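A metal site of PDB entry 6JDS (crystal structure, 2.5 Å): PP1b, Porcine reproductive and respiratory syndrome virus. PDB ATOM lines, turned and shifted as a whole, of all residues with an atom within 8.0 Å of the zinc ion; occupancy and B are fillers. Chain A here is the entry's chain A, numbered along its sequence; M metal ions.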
ATOM      1  N   MET A   6     -29.428 -17.805   1.005  1.00  0.00           N
ATOM      2  CA  MET A   6     -28.148 -17.739   0.307  1.00  0.00           C
ATOM      3  C   MET A   6     -27.411 -16.452   0.636  1.00  0.00           C
ATOM      4  O   MET A   6     -28.022 -15.430   0.936  1.00  0.00           O
ATOM      5  CB  MET A   6     -28.367 -17.852  -1.205  1.00  0.00           C
ATOM      6  CG  MET A   6     -29.059 -19.146  -1.631  1.00  0.00           C
ATOM      7  SD  MET A   6     -28.090 -20.629  -1.272  1.00  0.00           S
ATOM      8  CE  MET A   6     -29.380 -21.809  -0.891  1.00  0.00           C
ATOM      9  N   CYS A   7     -26.076 -16.510   0.573  1.00  0.00           N
ATOM     10  CA  CYS A   7     -25.244 -15.394   0.973  1.00  0.00           C
ATOM     11  C   CYS A   7     -25.416 -14.240   0.005  1.00  0.00           C
ATOM     12  O   CYS A   7     -25.390 -14.430  -1.208  1.00  0.00           O
ATOM     13  CB  CYS A   7     -23.771 -15.816   1.024  1.00  0.00           C
ATOM     14  SG  CYS A   7     -22.627 -14.476   1.427  1.00  0.00           S
ATOM     15  N   GLY A   8     -25.603 -13.039   0.553  1.00  0.00           N
ATOM     16  CA  GLY A   8     -25.837 -11.847  -0.249  1.00  0.00           C
ATOM     17  C   GLY A   8     -24.629 -11.403  -1.038  1.00  0.00           C
ATOM     18  O   GLY A   8     -24.753 -10.658  -2.000  1.00  0.00           O
ATOM     19  N   TYR A   9     -23.434 -11.847  -0.614  1.00  0.00           N
ATOM     20  CA  TYR A   9     -22.202 -11.557  -1.335  1.00  0.00           C
ATOM     21  C   TYR A   9     -21.945 -12.584  -2.450  1.00  0.00           C
ATOM     22  O   TYR A   9     -21.820 -12.221  -3.612  1.00  0.00           O
ATOM     23  CB  TYR A   9     -21.002 -11.561  -0.393  1.00  0.00           C
ATOM     24  CG  TYR A   9     -20.936 -10.398   0.578  1.00  0.00           C
ATOM     25  CD1 TYR A   9     -20.622  -9.117   0.136  1.00  0.00           C
ATOM     26  CD2 TYR A   9     -21.158 -10.594   1.948  1.00  0.00           C
ATOM     27  CE1 TYR A   9     -20.543  -8.058   1.028  1.00  0.00           C
ATOM     28  CE2 TYR A   9     -21.083  -9.536   2.831  1.00  0.00           C
ATOM     29  CZ  TYR A   9     -20.775  -8.268   2.371  1.00  0.00           C
ATOM     30  OH  TYR A   9     -20.700  -7.210   3.254  1.00  0.00           O
ATOM     31  N   CYS A  10     -21.861 -13.861  -2.066  1.00  0.00           N
ATOM     32  CA  CYS A  10     -21.345 -14.916  -2.951  1.00  0.00           C
ATOM     33  C   CYS A  10     -22.364 -15.979  -3.395  1.00  0.00           C
ATOM     34  O   CYS A  10     -22.061 -16.780  -4.288  1.00  0.00           O
ATOM     35  CB  CYS A  10     -20.172 -15.625  -2.267  1.00  0.00           C
ATOM     36  SG  CYS A  10     -20.659 -16.742  -0.930  1.00  0.00           S
ATOM     37  N   GLY A  11     -23.539 -16.019  -2.771  1.00  0.00           N
ATOM     38  CA  GLY A  11     -24.583 -16.961  -3.156  1.00  0.00           C
ATOM     39  C   GLY A  11     -24.534 -18.331  -2.499  1.00  0.00           C
ATOM     40  O   GLY A  11     -25.425 -19.151  -2.706  1.00  0.00           O
ATOM     41  N   ALA A  12     -23.501 -18.580  -1.688  1.00  0.00           N
ATOM     42  CA  ALA A  12     -23.375 -19.860  -0.979  1.00  0.00           C
ATOM     43  C   ALA A  12     -24.378 -19.907   0.167  1.00  0.00           C
ATOM     44  O   ALA A  12     -24.896 -18.861   0.578  1.00  0.00           O
ATOM     45  CB  ALA A  12     -21.963 -20.032  -0.450  1.00  0.00           C
ATOM     46  N   PRO A  13     -24.685 -21.119   0.696  1.00  0.00           N
ATOM     47  CA  PRO A  13     -25.612 -21.224   1.817  1.00  0.00           C
ATOM     48  C   PRO A  13     -25.266 -20.280   2.970  1.00  0.00           C
ATOM     49  O   PRO A  13     -24.094 -20.162   3.332  1.00  0.00           O
ATOM     50  CB  PRO A  13     -25.485 -22.684   2.253  1.00  0.00           C
ATOM     51  CG  PRO A  13     -25.112 -23.400   0.995  1.00  0.00           C
ATOM     52  CD  PRO A  13     -24.242 -22.450   0.217  1.00  0.00           C
ATOM     53  N   ALA A  14     -26.283 -19.610   3.518  1.00  0.00           N
ATOM     54  CA  ALA A  14     -26.097 -18.573   4.531  1.00  0.00           C
ATOM     55  C   ALA A  14     -26.880 -18.895   5.807  1.00  0.00           C
ATOM     56  O   ALA A  14     -28.068 -18.593   5.889  1.00  0.00           O
ATOM     57  CB  ALA A  14     -26.531 -17.232   3.974  1.00  0.00           C
ATOM     58  N   ASP A  23     -27.931 -11.658   4.476  1.00  0.00           N
ATOM     59  CA  ASP A  23     -27.570 -13.039   4.773  1.00  0.00           C
ATOM     60  C   ASP A  23     -26.126 -13.281   4.356  1.00  0.00           C
ATOM     61  O   ASP A  23     -25.698 -12.801   3.306  1.00  0.00           O
ATOM     62  CB  ASP A  23     -28.496 -14.010   4.040  1.00  0.00           C
ATOM     63  CG  ASP A  23     -29.940 -13.908   4.499  1.00  0.00           C
ATOM     64  OD1 ASP A  23     -30.170 -13.748   5.720  1.00  0.00           O
ATOM     65  OD2 ASP A  23     -30.849 -13.985   3.647  1.00  0.00           O
ATOM     66  N   VAL A  24     -25.387 -14.027   5.174  1.00  0.00           N
ATOM     67  CA  VAL A  24     -23.981 -14.299   4.879  1.00  0.00           C
ATOM     68  C   VAL A  24     -23.574 -15.731   5.207  1.00  0.00           C
ATOM     69  O   VAL A  24     -24.052 -16.317   6.185  1.00  0.00           O
ATOM     70  CB  VAL A  24     -23.023 -13.331   5.632  1.00  0.00           C
ATOM     71  CG1 VAL A  24     -23.122 -11.926   5.047  1.00  0.00           C
ATOM     72  CG2 VAL A  24     -23.323 -13.311   7.126  1.00  0.00           C
ATOM     73  N   CYS A  25     -22.692 -16.282   4.371  1.00  0.00           N
ATOM     74  CA  CYS A  25     -22.117 -17.605   4.595  1.00  0.00           C
ATOM     75  C   CYS A  25     -21.062 -17.517   5.689  1.00  0.00           C
ATOM     76  O   CYS A  25     -20.706 -16.419   6.141  1.00  0.00           O
ATOM     77  CB  CYS A  25     -21.501 -18.144   3.301  1.00  0.00           C
ATOM     78  SG  CYS A  25     -20.086 -17.198   2.699  1.00  0.00           S
ATOM     79  N   VAL A  26     -20.551 -18.678   6.096  1.00  0.00           N
ATOM     80  CA  VAL A  26     -19.516 -18.760   7.135  1.00  0.00           C
ATOM     81  C   VAL A  26     -18.341 -17.834   6.822  1.00  0.00           C
ATOM     82  O   VAL A  26     -17.866 -17.117   7.697  1.00  0.00           O
ATOM     83  CB  VAL A  26     -19.005 -20.212   7.298  1.00  0.00           C
ATOM     84  CG1 VAL A  26     -17.751 -20.271   8.169  1.00  0.00           C
ATOM     85  CG2 VAL A  26     -20.084 -21.102   7.895  1.00  0.00           C
ATOM     86  N   TYR A  27     -17.891 -17.861   5.571  1.00  0.00           N
ATOM     87  CA  TYR A  27     -16.759 -17.031   5.158  1.00  0.00           C
ATOM     88  C   TYR A  27     -17.054 -15.537   5.346  1.00  0.00           C
ATOM     89  O   TYR A  27     -16.270 -14.825   5.972  1.00  0.00           O
ATOM     90  CB  TYR A  27     -16.377 -17.309   3.699  1.00  0.00           C
ATOM     91  CG  TYR A  27     -15.223 -16.469   3.219  1.00  0.00           C
ATOM     92  CD1 TYR A  27     -13.913 -16.772   3.581  1.00  0.00           C
ATOM     93  CD2 TYR A  27     -15.430 -15.343   2.404  1.00  0.00           C
ATOM     94  CE1 TYR A  27     -12.845 -16.007   3.151  1.00  0.00           C
ATOM     95  CE2 TYR A  27     -14.377 -14.571   1.969  1.00  0.00           C
ATOM     96  CZ  TYR A  27     -13.079 -14.907   2.341  1.00  0.00           C
ATOM     97  OH  TYR A  27     -12.017 -14.142   1.925  1.00  0.00           O
ATOM     98  N   HIS A  28     -18.181 -15.075   4.812  1.00  0.00           N
ATOM     99  CA  HIS A  28     -18.499 -13.648   4.788  1.00  0.00           C
ATOM    100  C   HIS A  28     -19.017 -13.079   6.111  1.00  0.00           C
ATOM    101  O   HIS A  28     -19.349 -11.894   6.185  1.00  0.00           O
ATOM    102  CB  HIS A  28     -19.463 -13.314   3.635  1.00  0.00           C
ATOM    103  CG  HIS A  28     -18.769 -13.176   2.316  1.00  0.00           C
ATOM    104  ND1 HIS A  28     -18.847 -14.139   1.320  1.00  0.00           N
ATOM    105  CD2 HIS A  28     -17.970 -12.202   1.821  1.00  0.00           C
ATOM    106  CE1 HIS A  28     -18.133 -13.745   0.276  1.00  0.00           C
ATOM    107  NE2 HIS A  28     -17.586 -12.580   0.564  1.00  0.00           N
ATOM    108  N   THR A  29     -19.086 -13.897   7.161  1.00  0.00           N
ATOM    109  CA  THR A  29     -19.356 -13.389   8.513  1.00  0.00           C
ATOM    110  C   THR A  29     -18.250 -12.448   9.004  1.00  0.00           C
ATOM    111  O   THR A  29     -18.504 -11.590   9.854  1.00  0.00           O
ATOM    112  CB  THR A  29     -19.511 -14.510   9.558  1.00  0.00           C
ATOM    113  OG1 THR A  29     -18.334 -15.342   9.549  1.00  0.00           O
ATOM    114  CG2 THR A  29     -20.734 -15.369   9.274  1.00  0.00           C
ATOM    115  N   VAL A 135     -24.561 -11.302  -6.387  1.00  0.00           N
ATOM    116  CA  VAL A 135     -24.350 -12.186  -7.524  1.00  0.00           C
ATOM    117  C   VAL A 135     -25.379 -11.871  -8.612  1.00  0.00           C
ATOM    118  O   VAL A 135     -25.032 -11.731  -9.786  1.00  0.00           O
ATOM    119  CB  VAL A 135     -24.443 -13.680  -7.116  1.00  0.00           C
ATOM    120  CG1 VAL A 135     -24.386 -14.580  -8.348  1.00  0.00           C
ATOM    121  CG2 VAL A 135     -23.329 -14.037  -6.149  1.00  0.00           C
HETATM  122 ZN    ZN M   1     -20.608 -15.539   1.105  1.00  0.00          ZN
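The backbone NH of Tyr 9 sits close to the side-chain sulfur of Cys 7, 3.4 Å away.
N of Cys 7 sits at hydrogen-bond distance from O of Ala 12, at 2.6 Å.
SG of Cys 25 sits close to N of Tyr 27 (3.7 Å).
The backbone NH (N) of Ala 12 lies close to the side-chain sulfur (SG) of Cys 10, at 3.5 Å.
The nearest printed residue that does not touch the zinc ion is Tyr 9 (4.3 Å).
The zinc ion is bound by a ring nitrogen (ND1) of His 28 (2.3 Å).
SG of Cys 7 binds the zinc ion, at 2.3 Å.
The zinc ion is bound by SG of Cys 25, at 2.4 Å.
The zinc ion is bound by the side-chain sulfur (SG) of Cys 10 (2.4 Å).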
